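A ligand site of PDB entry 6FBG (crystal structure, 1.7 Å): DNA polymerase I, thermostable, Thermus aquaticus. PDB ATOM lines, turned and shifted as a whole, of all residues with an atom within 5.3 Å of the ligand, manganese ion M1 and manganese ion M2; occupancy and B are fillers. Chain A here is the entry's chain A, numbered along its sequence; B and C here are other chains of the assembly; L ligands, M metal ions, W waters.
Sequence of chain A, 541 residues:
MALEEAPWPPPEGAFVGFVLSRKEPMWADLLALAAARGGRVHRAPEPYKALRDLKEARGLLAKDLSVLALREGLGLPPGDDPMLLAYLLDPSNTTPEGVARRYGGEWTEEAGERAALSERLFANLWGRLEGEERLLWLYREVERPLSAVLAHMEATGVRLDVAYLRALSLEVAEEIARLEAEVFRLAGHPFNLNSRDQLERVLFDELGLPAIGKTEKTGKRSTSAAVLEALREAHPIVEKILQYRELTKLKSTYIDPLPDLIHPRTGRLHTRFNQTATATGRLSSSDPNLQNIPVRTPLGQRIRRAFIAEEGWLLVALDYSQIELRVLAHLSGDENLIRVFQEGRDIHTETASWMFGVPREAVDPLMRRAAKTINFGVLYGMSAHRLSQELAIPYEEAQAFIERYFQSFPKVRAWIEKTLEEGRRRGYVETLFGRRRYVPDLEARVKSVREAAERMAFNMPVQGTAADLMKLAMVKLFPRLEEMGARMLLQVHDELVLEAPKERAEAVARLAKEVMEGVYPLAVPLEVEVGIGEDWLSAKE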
ATOM      1  N   ARG A 282      -1.066  26.297  14.261  1.00  0.00           N
ATOM      2  CA  ARG A 282      -1.837  25.366  13.453  1.00  0.00           C
ATOM      3  C   ARG A 282      -3.320  25.459  13.802  1.00  0.00           C
ATOM      4  O   ARG A 282      -3.692  25.805  14.921  1.00  0.00           O
ATOM      5  CB  ARG A 282      -1.364  23.933  13.667  1.00  0.00           C
ATOM      6  CG  ARG A 282      -0.183  23.486  12.840  1.00  0.00           C
ATOM      7  CD  ARG A 282      -0.009  21.986  13.004  1.00  0.00           C
ATOM      8  NE  ARG A 282       0.961  21.407  12.086  1.00  0.00           N
ATOM      9  CZ  ARG A 282       1.166  20.100  11.966  1.00  0.00           C
ATOM     10  NH1 ARG A 282       0.489  19.245  12.705  1.00  0.00           N
ATOM     11  NH2 ARG A 282       2.066  19.652  11.101  1.00  0.00           N
ATOM     12  N   ASP A 319      -0.801  19.835  -1.788  1.00  0.00           N
ATOM     13  CA  ASP A 319       0.004  19.557  -0.598  1.00  0.00           C
ATOM     14  C   ASP A 319       1.410  20.107  -0.803  1.00  0.00           C
ATOM     15  O   ASP A 319       2.083  19.733  -1.772  1.00  0.00           O
ATOM     16  CB  ASP A 319       0.036  18.061  -0.315  1.00  0.00           C
ATOM     17  CG  ASP A 319       0.749  17.723   0.968  1.00  0.00           C
ATOM     18  OD1 ASP A 319       1.949  18.038   1.073  1.00  0.00           O
ATOM     19  OD2 ASP A 319       0.108  17.159   1.872  1.00  0.00           O
ATOM     20  N   TYR A 320       1.852  20.971   0.107  1.00  0.00           N
ATOM     21  CA  TYR A 320       3.196  21.536   0.013  1.00  0.00           C
ATOM     22  C   TYR A 320       4.248  20.433   0.140  1.00  0.00           C
ATOM     23  O   TYR A 320       4.146  19.555   0.993  1.00  0.00           O
ATOM     24  CB  TYR A 320       3.419  22.586   1.108  1.00  0.00           C
ATOM     25  CG  TYR A 320       2.787  23.937   0.858  1.00  0.00           C
ATOM     26  CD1 TYR A 320       3.356  24.846  -0.034  1.00  0.00           C
ATOM     27  CD2 TYR A 320       1.638  24.324   1.530  1.00  0.00           C
ATOM     28  CE1 TYR A 320       2.786  26.092  -0.253  1.00  0.00           C
ATOM     29  CE2 TYR A 320       1.058  25.560   1.307  1.00  0.00           C
ATOM     30  CZ  TYR A 320       1.634  26.441   0.420  1.00  0.00           C
ATOM     31  OH  TYR A 320       1.057  27.672   0.205  1.00  0.00           O
ATOM     32  N   SER A 321       5.257  20.506  -0.720  1.00  0.00           N
ATOM     33  CA  SER A 321       6.359  19.547  -0.703  1.00  0.00           C
ATOM     34  C   SER A 321       7.336  19.863   0.428  1.00  0.00           C
ATOM     35  O   SER A 321       7.816  20.994   0.541  1.00  0.00           O
ATOM     36  CB  SER A 321       7.085  19.558  -2.049  1.00  0.00           C
ATOM     37  OG  SER A 321       8.344  18.914  -1.960  1.00  0.00           O
ATOM     38  N   GLN A 322       7.631  18.859   1.250  1.00  0.00           N
ATOM     39  CA  GLN A 322       8.705  18.938   2.256  1.00  0.00           C
ATOM     40  C   GLN A 322       8.673  20.269   2.992  1.00  0.00           C
ATOM     41  O   GLN A 322       9.688  20.950   3.139  1.00  0.00           O
ATOM     42  CB  GLN A 322      10.066  18.737   1.583  1.00  0.00           C
ATOM     43  CG  GLN A 322      10.131  17.584   0.603  1.00  0.00           C
ATOM     44  CD  GLN A 322      11.468  17.538  -0.118  1.00  0.00           C
ATOM     45  OE1 GLN A 322      12.480  17.117   0.448  1.00  0.00           O
ATOM     46  NE2 GLN A 322      11.483  17.974  -1.375  1.00  0.00           N
ATOM     47  N   ILE A 323       7.487  20.643   3.490  1.00  0.00           N
ATOM     48  CA  ILE A 323       7.237  22.045   3.783  1.00  0.00           C
ATOM     49  C   ILE A 323       8.117  22.531   4.928  1.00  0.00           C
ATOM     50  O   ILE A 323       8.768  23.577   4.829  1.00  0.00           O
ATOM     51  CB  ILE A 323       5.745  22.294   4.053  1.00  0.00           C
ATOM     52  CG1 ILE A 323       5.488  23.785   4.308  1.00  0.00           C
ATOM     53  CG2 ILE A 323       5.231  21.463   5.220  1.00  0.00           C
ATOM     54  CD1 ILE A 323       5.905  24.689   3.152  1.00  0.00           C
ATOM     55  N   GLU A 324       8.167  21.796   6.041  1.00  0.00           N
ATOM     56  CA  GLU A 324       8.917  22.308   7.190  1.00  0.00           C
ATOM     57  C   GLU A 324      10.424  22.294   6.938  1.00  0.00           C
ATOM     58  O   GLU A 324      11.146  23.093   7.532  1.00  0.00           O
ATOM     59  CB  GLU A 324       8.561  21.524   8.458  1.00  0.00           C
ATOM     60  CG  GLU A 324       7.278  22.074   9.115  1.00  0.00           C
ATOM     61  CD  GLU A 324       6.959  21.452  10.470  1.00  0.00           C
ATOM     62  OE1 GLU A 324       7.899  21.017  11.168  1.00  0.00           O
ATOM     63  OE2 GLU A 324       5.762  21.389  10.821  1.00  0.00           O
ATOM     64  N   LEU A 325      10.906  21.427   6.039  1.00  0.00           N
ATOM     65  CA  LEU A 325      12.310  21.506   5.648  1.00  0.00           C
ATOM     66  C   LEU A 325      12.577  22.744   4.805  1.00  0.00           C
ATOM     67  O   LEU A 325      13.603  23.411   4.990  1.00  0.00           O
ATOM     68  CB  LEU A 325      12.718  20.243   4.883  1.00  0.00           C
ATOM     69  CG  LEU A 325      12.688  18.942   5.695  1.00  0.00           C
ATOM     70  CD1 LEU A 325      13.016  17.745   4.815  1.00  0.00           C
ATOM     71  CD2 LEU A 325      13.637  19.009   6.880  1.00  0.00           C
ATOM     72  N   HIS A 348      13.169  13.397   1.614  1.00  0.00           N
ATOM     73  CA  HIS A 348      12.437  12.214   2.068  1.00  0.00           C
ATOM     74  C   HIS A 348      12.805  11.001   1.213  1.00  0.00           C
ATOM     75  O   HIS A 348      13.103   9.924   1.741  1.00  0.00           O
ATOM     76  CB  HIS A 348      10.939  12.466   2.024  1.00  0.00           C
ATOM     77  CG  HIS A 348      10.475  13.510   2.988  1.00  0.00           C
ATOM     78  ND1 HIS A 348      11.172  13.825   4.133  1.00  0.00           N
ATOM     79  CD2 HIS A 348       9.379  14.311   2.986  1.00  0.00           C
ATOM     80  CE1 HIS A 348      10.535  14.780   4.794  1.00  0.00           C
ATOM     81  NE2 HIS A 348       9.439  15.090   4.118  1.00  0.00           N
ATOM     82  N   ARG A 368       8.824   6.171   1.521  1.00  0.00           N
ATOM     83  CA  ARG A 368       9.050   7.606   1.634  1.00  0.00           C
ATOM     84  C   ARG A 368       8.365   8.173   2.883  1.00  0.00           C
ATOM     85  O   ARG A 368       8.914   9.063   3.542  1.00  0.00           O
ATOM     86  CB  ARG A 368       8.555   8.320   0.379  1.00  0.00           C
ATOM     87  CG  ARG A 368       8.915   9.786   0.323  1.00  0.00           C
ATOM     88  CD  ARG A 368       8.565  10.412  -1.022  1.00  0.00           C
ATOM     89  NE  ARG A 368       8.900  11.832  -1.049  1.00  0.00           N
ATOM     90  CZ  ARG A 368       8.137  12.793  -0.528  1.00  0.00           C
ATOM     91  NH1 ARG A 368       6.994  12.485   0.065  1.00  0.00           N
ATOM     92  NH2 ARG A 368       8.527  14.060  -0.594  1.00  0.00           N
ATOM     93  N   ARG A 369       7.175   7.665   3.202  1.00  0.00           N
ATOM     94  CA  ARG A 369       6.492   8.094   4.418  1.00  0.00           C
ATOM     95  C   ARG A 369       7.308   7.768   5.659  1.00  0.00           C
ATOM     96  O   ARG A 369       7.435   8.590   6.567  1.00  0.00           O
ATOM     97  CB  ARG A 369       5.107   7.449   4.484  1.00  0.00           C
ATOM     98  CG  ARG A 369       4.470   7.494   5.861  1.00  0.00           C
ATOM     99  CD  ARG A 369       2.997   7.123   5.795  1.00  0.00           C
ATOM    100  NE  ARG A 369       2.219   8.131   5.066  1.00  0.00           N
ATOM    101  CZ  ARG A 369       1.742   9.250   5.616  1.00  0.00           C
ATOM    102  NH1 ARG A 369       1.057  10.102   4.872  1.00  0.00           N
ATOM    103  NH2 ARG A 369       1.947   9.513   6.896  1.00  0.00           N
ATOM    104  N   LYS A 372      10.063  10.258   5.935  1.00  0.00           N
ATOM    105  CA  LYS A 372       9.577  11.532   6.456  1.00  0.00           C
ATOM    106  C   LYS A 372       9.621  11.534   7.983  1.00  0.00           C
ATOM    107  O   LYS A 372      10.091  12.501   8.597  1.00  0.00           O
ATOM    108  CB  LYS A 372       8.148  11.771   5.956  1.00  0.00           C
ATOM    109  CG  LYS A 372       7.473  13.032   6.513  1.00  0.00           C
ATOM    110  CD  LYS A 372       6.006  12.769   6.863  1.00  0.00           C
ATOM    111  CE  LYS A 372       5.876  11.891   8.109  1.00  0.00           C
ATOM    112  NZ  LYS A 372       4.488  11.897   8.656  1.00  0.00           N
ATOM    113  N   THR A 373       9.132  10.466   8.606  1.00  0.00           N
ATOM    114  CA  THR A 373       9.137  10.382  10.062  1.00  0.00           C
ATOM    115  C   THR A 373      10.560  10.457  10.604  1.00  0.00           C
ATOM    116  O   THR A 373      10.815  11.127  11.614  1.00  0.00           O
ATOM    117  CB  THR A 373       8.447   9.089  10.501  1.00  0.00           C
ATOM    118  OG1 THR A 373       7.132   9.039   9.949  1.00  0.00           O
ATOM    119  CG2 THR A 373       8.360   9.005  12.017  1.00  0.00           C
ATOM    120  N   PHE A 376      12.126  14.256  10.197  1.00  0.00           N
ATOM    121  CA  PHE A 376      11.660  15.228  11.175  1.00  0.00           C
ATOM    122  C   PHE A 376      11.909  14.766  12.609  1.00  0.00           C
ATOM    123  O   PHE A 376      12.164  15.594  13.485  1.00  0.00           O
ATOM    124  CB  PHE A 376      10.171  15.510  10.970  1.00  0.00           C
ATOM    125  CG  PHE A 376       9.890  16.221   9.684  1.00  0.00           C
ATOM    126  CD1 PHE A 376      10.373  17.496   9.475  1.00  0.00           C
ATOM    127  CD2 PHE A 376       9.151  15.615   8.683  1.00  0.00           C
ATOM    128  CE1 PHE A 376      10.135  18.159   8.293  1.00  0.00           C
ATOM    129  CE2 PHE A 376       8.891  16.271   7.491  1.00  0.00           C
ATOM    130  CZ  PHE A 376       9.389  17.546   7.302  1.00  0.00           C
ATOM    131  N   GLY A 377      11.862  13.459  12.862  1.00  0.00           N
ATOM    132  CA  GLY A 377      12.238  12.968  14.177  1.00  0.00           C
ATOM    133  C   GLY A 377      13.647  13.378  14.562  1.00  0.00           C
ATOM    134  O   GLY A 377      13.884  13.886  15.657  1.00  0.00           O
ATOM    135  N   TYR A 380      14.028  17.295  15.163  1.00  0.00           N
ATOM    136  CA  TYR A 380      13.473  17.824  16.388  1.00  0.00           C
ATOM    137  C   TYR A 380      13.886  17.028  17.617  1.00  0.00           C
ATOM    138  O   TYR A 380      13.229  17.114  18.661  1.00  0.00           O
ATOM    139  CB  TYR A 380      11.940  17.909  16.266  1.00  0.00           C
ATOM    140  CG  TYR A 380      11.503  18.843  15.155  1.00  0.00           C
ATOM    141  CD1 TYR A 380      11.865  20.189  15.181  1.00  0.00           C
ATOM    142  CD2 TYR A 380      10.738  18.391  14.092  1.00  0.00           C
ATOM    143  CE1 TYR A 380      11.478  21.048  14.178  1.00  0.00           C
ATOM    144  CE2 TYR A 380      10.348  19.255  13.081  1.00  0.00           C
ATOM    145  CZ  TYR A 380      10.719  20.585  13.131  1.00  0.00           C
ATOM    146  OH  TYR A 380      10.331  21.452  12.133  1.00  0.00           O
ATOM    147  N   ASN A 459      10.925  23.882  17.634  1.00  0.00           N
ATOM    148  CA  ASN A 459       9.964  23.365  16.663  1.00  0.00           C
ATOM    149  C   ASN A 459       8.937  24.421  16.277  1.00  0.00           C
ATOM    150  O   ASN A 459       8.526  24.498  15.107  1.00  0.00           O
ATOM    151  CB  ASN A 459       9.259  22.133  17.239  1.00  0.00           C
ATOM    152  CG  ASN A 459       8.059  21.702  16.404  1.00  0.00           C
ATOM    153  OD1 ASN A 459       6.942  22.173  16.600  1.00  0.00           O
ATOM    154  ND2 ASN A 459       8.297  20.795  15.454  1.00  0.00           N
ATOM    155  N   VAL A 492      -5.595  20.313   5.837  1.00  0.00           N
ATOM    156  CA  VAL A 492      -4.900  19.316   6.629  1.00  0.00           C
ATOM    157  C   VAL A 492      -3.469  19.803   6.857  1.00  0.00           C
ATOM    158  O   VAL A 492      -2.503  19.146   6.460  1.00  0.00           O
ATOM    159  CB  VAL A 492      -4.949  17.937   5.954  1.00  0.00           C
ATOM    160  CG1 VAL A 492      -4.461  16.844   6.897  1.00  0.00           C
ATOM    161  CG2 VAL A 492      -6.382  17.614   5.498  1.00  0.00           C
ATOM    162  N   ASP A 494      -0.833  21.317   5.822  1.00  0.00           N
ATOM    163  CA  ASP A 494      -0.134  21.819   4.649  1.00  0.00           C
ATOM    164  C   ASP A 494      -0.812  21.370   3.365  1.00  0.00           C
ATOM    165  O   ASP A 494      -0.184  21.347   2.300  1.00  0.00           O
ATOM    166  CB  ASP A 494       1.342  21.394   4.657  1.00  0.00           C
ATOM    167  CG  ASP A 494       1.537  19.974   4.143  1.00  0.00           C
ATOM    168  OD1 ASP A 494       0.642  19.131   4.335  1.00  0.00           O
ATOM    169  OD2 ASP A 494       2.604  19.711   3.550  1.00  0.00           O
ATOM    170  N   GLU A 495      -2.096  21.011   3.453  1.00  0.00           N
ATOM    171  CA  GLU A 495      -2.844  20.474   2.338  1.00  0.00           C
ATOM    172  C   GLU A 495      -4.222  21.096   2.303  1.00  0.00           C
ATOM    173  O   GLU A 495      -4.820  21.353   3.355  1.00  0.00           O
ATOM    174  CB  GLU A 495      -2.958  18.937   2.443  1.00  0.00           C
ATOM    175  CG  GLU A 495      -4.014  18.303   1.541  1.00  0.00           C
ATOM    176  CD  GLU A 495      -4.161  16.815   1.781  1.00  0.00           C
ATOM    177  OE1 GLU A 495      -3.526  16.296   2.726  1.00  0.00           O
ATOM    178  OE2 GLU A 495      -4.911  16.169   1.024  1.00  0.00           O
ATOM    179  P    DC B  12      -1.290  12.297   6.498  1.00  0.00           P
ATOM    180  OP1  DC B  12      -1.773  12.599   5.130  1.00  0.00           O
ATOM    181  OP2  DC B  12      -0.237  11.290   6.717  1.00  0.00           O
ATOM    182  O5'  DC B  12      -0.813  13.672   7.164  1.00  0.00           O
ATOM    183  C5'  DC B  12      -1.611  14.852   7.035  1.00  0.00           C
ATOM    184  C4'  DC B  12      -0.973  16.016   7.749  1.00  0.00           C
ATOM    185  O4'  DC B  12      -0.879  15.719   9.164  1.00  0.00           O
ATOM    186  C3'  DC B  12       0.455  16.332   7.322  1.00  0.00           C
ATOM    187  O3'  DC B  12       0.458  17.222   6.221  1.00  0.00           O
ATOM    188  C2'  DC B  12       1.071  16.936   8.572  1.00  0.00           C
ATOM    189  C1'  DC B  12       0.274  16.325   9.718  1.00  0.00           C
ATOM    190  N1   DC B  12       1.028  15.282  10.494  1.00  0.00           N
ATOM    191  C2   DC B  12       1.754  15.646  11.624  1.00  0.00           C
ATOM    192  O2   DC B  12       1.769  16.842  11.968  1.00  0.00           O
ATOM    193  N3   DC B  12       2.418  14.684  12.313  1.00  0.00           N
ATOM    194  C4   DC B  12       2.364  13.418  11.909  1.00  0.00           C
ATOM    195  N4   DC B  12       3.045  12.501  12.622  1.00  0.00           N
ATOM    196  C5   DC B  12       1.630  13.019  10.757  1.00  0.00           C
ATOM    197  C6   DC B  12       0.981  13.980  10.088  1.00  0.00           C
ATOM    198  P    DC C   4      12.838  10.435  21.747  1.00  0.00           P
ATOM    199  OP1  DC C   4      11.703   9.504  21.903  1.00  0.00           O
ATOM    200  OP2  DC C   4      14.201   9.910  21.524  1.00  0.00           O
ATOM    201  O5'  DC C   4      12.484  11.445  20.569  1.00  0.00           O
ATOM    202  C5'  DC C   4      11.341  12.288  20.677  1.00  0.00           C
ATOM    203  C4'  DC C   4      11.528  13.565  19.892  1.00  0.00           C
ATOM    204  O4'  DC C   4      11.749  13.251  18.495  1.00  0.00           O
ATOM    205  C3'  DC C   4      10.333  14.506  19.909  1.00  0.00           C
ATOM    206  O3'  DC C   4      10.388  15.393  21.030  1.00  0.00           O
ATOM    207  C2'  DC C   4      10.459  15.232  18.584  1.00  0.00           C
ATOM    208  C1'  DC C   4      11.044  14.160  17.670  1.00  0.00           C
ATOM    209  N1   DC C   4      10.023  13.400  16.896  1.00  0.00           N
ATOM    210  C2   DC C   4       9.332  14.030  15.859  1.00  0.00           C
ATOM    211  O2   DC C   4       9.592  15.220  15.597  1.00  0.00           O
ATOM    212  N3   DC C   4       8.407  13.334  15.157  1.00  0.00           N
ATOM    213  C4   DC C   4       8.154  12.064  15.463  1.00  0.00           C
ATOM    214  N4   DC C   4       7.238  11.413  14.751  1.00  0.00           N
ATOM    215  C5   DC C   4       8.848  11.393  16.521  1.00  0.00           C
ATOM    216  C6   DC C   4       9.757  12.098  17.209  1.00  0.00           C
ATOM    217  P    DG C   5       9.070  15.728  21.881  1.00  0.00           P
ATOM    218  OP1  DG C   5       9.494  16.395  23.132  1.00  0.00           O
ATOM    219  OP2  DG C   5       8.238  14.497  21.932  1.00  0.00           O
ATOM    220  O5'  DG C   5       8.293  16.791  20.974  1.00  0.00           O
ATOM    221  C5'  DG C   5       8.882  18.065  20.725  1.00  0.00           C
ATOM    222  C4'  DG C   5       8.161  18.801  19.607  1.00  0.00           C
ATOM    223  O4'  DG C   5       8.296  18.041  18.378  1.00  0.00           O
ATOM    224  C3'  DG C   5       6.669  18.972  19.798  1.00  0.00           C
ATOM    225  O3'  DG C   5       6.385  20.131  20.597  1.00  0.00           O
ATOM    226  C2'  DG C   5       6.168  19.106  18.370  1.00  0.00           C
ATOM    227  C1'  DG C   5       7.142  18.236  17.567  1.00  0.00           C
ATOM    228  N9   DG C   5       6.585  16.925  17.217  1.00  0.00           N
ATOM    229  C8   DG C   5       6.884  15.718  17.807  1.00  0.00           C
ATOM    230  N7   DG C   5       6.240  14.711  17.268  1.00  0.00           N
ATOM    231  C5   DG C   5       5.473  15.299  16.268  1.00  0.00           C
ATOM    232  C6   DG C   5       4.568  14.714  15.344  1.00  0.00           C
ATOM    233  O6   DG C   5       4.248  13.520  15.230  1.00  0.00           O
ATOM    234  N1   DG C   5       4.006  15.671  14.499  1.00  0.00           N
ATOM    235  C2   DG C   5       4.280  17.012  14.542  1.00  0.00           C
ATOM    236  N2   DG C   5       3.642  17.788  13.651  1.00  0.00           N
ATOM    237  N3   DG C   5       5.121  17.578  15.401  1.00  0.00           N
ATOM    238  C4   DG C   5       5.680  16.662  16.224  1.00  0.00           C
HETATM  239  N1  LIG L   1       7.099  14.669  13.057  1.00  0.00           N
HETATM  240  C1  LIG L   1       7.160  16.033  13.068  1.00  0.00           C
HETATM  241  N2  LIG L   1       7.879  16.608  14.042  1.00  0.00           N
HETATM  242  N3  LIG L   1       6.555  16.802  12.172  1.00  0.00           N
HETATM  243  C2  LIG L   1       5.859  16.087  11.257  1.00  0.00           C
HETATM  244  C3  LIG L   1       5.721  14.716  11.181  1.00  0.00           C
HETATM  245  C4  LIG L   1       6.394  13.909  12.153  1.00  0.00           C
HETATM  246  O1  LIG L   1       6.401  12.683  12.213  1.00  0.00           O
HETATM  247  N4  LIG L   1       4.917  14.376  10.097  1.00  0.00           N
HETATM  248  C5  LIG L   1       4.618  15.522   9.541  1.00  0.00           C
HETATM  249  N5  LIG L   1       5.166  16.603  10.192  1.00  0.00           N
HETATM  250  P1  LIG L   1       3.471  16.040   5.142  1.00  0.00           P
HETATM  251  P2  LIG L   1       6.044  16.826   3.916  1.00  0.00           P
HETATM  252  P3  LIG L   1       5.723  15.800   1.217  1.00  0.00           P
HETATM  253  C6  LIG L   1       5.175  18.007   9.766  1.00  0.00           C
HETATM  254  O2  LIG L   1       2.683  16.717   4.136  1.00  0.00           O
HETATM  255  O3  LIG L   1       5.448  18.121   3.677  1.00  0.00           O
HETATM  256  O4  LIG L   1       6.571  16.198   0.045  1.00  0.00           O
HETATM  257  C7  LIG L   1       6.417  18.369   8.969  1.00  0.00           C
HETATM  258  O5  LIG L   1       2.833  14.625   5.413  1.00  0.00           O
HETATM  259  O6  LIG L   1       7.313  17.021   4.828  1.00  0.00           O
HETATM  260  O7  LIG L   1       5.390  14.321   1.241  1.00  0.00           O
HETATM  261  C8  LIG L   1       5.946  18.206   7.527  1.00  0.00           C
HETATM  262  O8  LIG L   1       6.712  19.033   6.645  1.00  0.00           O
HETATM  263  N6  LIG L   1       5.019  15.805   4.669  1.00  0.00           N
HETATM  264  O9  LIG L   1       6.512  16.103   2.575  1.00  0.00           O
HETATM  265  O10 LIG L   1       4.420  16.593   1.312  1.00  0.00           O
HETATM  266  C9  LIG L   1       4.510  18.702   7.630  1.00  0.00           C
HETATM  267  O11 LIG L   1       4.052  18.219   8.917  1.00  0.00           O
HETATM  268  C10 LIG L   1       3.576  18.233   6.542  1.00  0.00           C
HETATM  269  O12 LIG L   1       3.539  16.792   6.520  1.00  0.00           O
HETATM  270 MN    MN M   1       3.562  18.138   2.454  1.00  0.00          MN
HETATM  271 MN    MN M   2       0.487  17.038   3.992  1.00  0.00          MN
HETATM  272  O   HOH W   1       2.244  12.367   7.066  1.00  0.00           O
HETATM  273  O   HOH W   2       0.395  14.814   4.043  1.00  0.00           O
HETATM  274  O   HOH W   3       3.508  21.602   9.260  1.00  0.00           O
HETATM  275  O   HOH W   4       3.552  17.383  -1.179  1.00  0.00           O
HETATM  276  O   HOH W   5       6.545  19.763  13.335  1.00  0.00           O
HETATM  277  O   HOH W   6      -1.640  16.797   4.361  1.00  0.00           O
HETATM  278  O   HOH W   7       5.186  10.603  11.114  1.00  0.00           O
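A nitrogen (N2) of the ligand is in hydrogen-bond range of O2 of DC 4 of chain C (2.7 Å).
O7 of the ligand is in salt-bridge range of NH1 of Arg 368 (2.7 Å).
The side-chain amino group of Lys 372 sits at hydrogen-bond distance from a nitrogen (N4) of the ligand (2.9 Å).
O6 of the ligand sits at hydrogen-bond distance from NE2 of His 348, at 3.0 Å.
N2 of the ligand sits close to N3 of DG 5 of chain C.
O4 of the ligand lies within hydrogen-bond range of N of Gln 322, at 3.1 Å.
The backbone NH of Glu 324 sits at hydrogen-bond distance from an oxygen (O8) of the ligand (3.2 Å).
An oxygen (O3) of the ligand sits close to the backbone NH (N) of Ile 323 (3.2 Å).
The guanidinium group of Arg 282 lies within hydrogen-bond range of an oxygen (O11) of the ligand (3.3 Å).
O2 of DC 12 of chain B sits close to N2 of DG 5 of chain C (2.7 Å).
O2 of DC 12 of chain B sits at hydrogen-bond distance from the guanidinium group (NH1) of Arg 282 (2.8 Å).
OP2 of DC 12 of chain B lies within salt-bridge range of NH1 of Arg 369 (2.5 Å).
The side-chain amide nitrogen of Gln 322 sits at hydrogen-bond distance from the side-chain hydroxyl of Ser 321, at 3.3 Å.
The side-chain carboxylate of Glu 324 is in hydrogen-bond range of the side-chain hydroxyl of Tyr 380, 2.7 Å away.
Ser 321 touches the ligand.
Phe 376 touches the ligand (CZ to O8, 3.1 Å).
Tyr 380 touches the ligand.
Hydrophobic or aromatic side chains that line the ligand: Ile 323, His 348, Phe 376 and Tyr 380.
Within 4 Å of the ligand: Arg 282, Asp 319, Tyr 320, Ser 321, Gln 322, Ile 323, Glu 324, His 348, Arg 368, Lys 372, Phe 376, Tyr 380, Asp 494, DC 12 of chain B, DC 4 of chain C and DG 5 of chain C.
The nearest printed residue that does not touch the ligand is Thr 373 (4.2 Å).
Of the 23 residues printed, 3 come within 4 Å of manganese ion M1.
Along chain A the residues within 4 Å of manganese ion M1 span positions 319 to 494.
The nearest printed residue that does not touch manganese ion M1 is Gln 322 (4.3 Å).
Three residues have an atom within 4 Å of manganese ion M2: Asp 319, Asp 494 and DC 12 of chain B.
Manganese ion M1 is bound by an oxygen (O10) of the ligand, 2.1 Å away.
Manganese ion M1 is bound by O of Tyr 320.
Manganese ion M1 is bound by OD1 of Asp 319 (2.1 Å).
The side-chain carboxylate (OD2) of Asp 494 is bound to manganese ion M1 (2.1 Å).
O3 of the ligand binds manganese ion M1, at 2.2 Å.
O2 of the ligand binds manganese ion M1 (2.4 Å).
Manganese ion M1 has six donor atoms within binding distance.
Manganese ion M2 is bound by the side-chain carboxylate (OD1) of Asp 494 (2.1 Å).
OD2 of Asp 319 is bound to manganese ion M2.
Water W6 is bound to manganese ion M2.
O2 of the ligand is bound to manganese ion M2 (2.2 Å).
Manganese ion M2 is bound by water W2, at 2.2 Å.
Manganese ion M2 is bound by O3' of DC 12 of chain B (2.2 Å).
Manganese ion M2 has six donor atoms within binding distance.
Water W6 lies within hydrogen-bond range of the side-chain carboxylate of Glu 495 (2.5 Å) and the backbone carbonyl oxygen of Val 492 (3.3 Å).
Water W2 lies within hydrogen-bond range of O5 of the ligand (2.8 Å) and OP1 of DC 12 of chain B (3.3 Å).
Water W7 lies within hydrogen-bond range of an oxygen (O1) of the ligand (2.6 Å), the side-chain hydroxyl (OG1) of Thr 373 (2.8 Å), the side-chain amino group (NZ) of Lys 372 (2.9 Å) and N4 of DC 12 of chain B (3.2 Å).
Water W4 bridges the backbone carbonyl oxygen of Asp 319 and an oxygen (O4) of the ligand.
Water W1 lies within hydrogen-bond range of OP2 of DC 12 of chain B (2.7 Å), the side-chain amino group (NZ) of Lys 372 (2.8 Å), an oxygen (O5) of the ligand (2.9 Å) and the guanidinium group (NH2) of Arg 369 (2.9 Å).
Water W3 lies within hydrogen-bond range of OE2 of Glu 324, NH2 of Arg 282 and O11 of the ligand.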
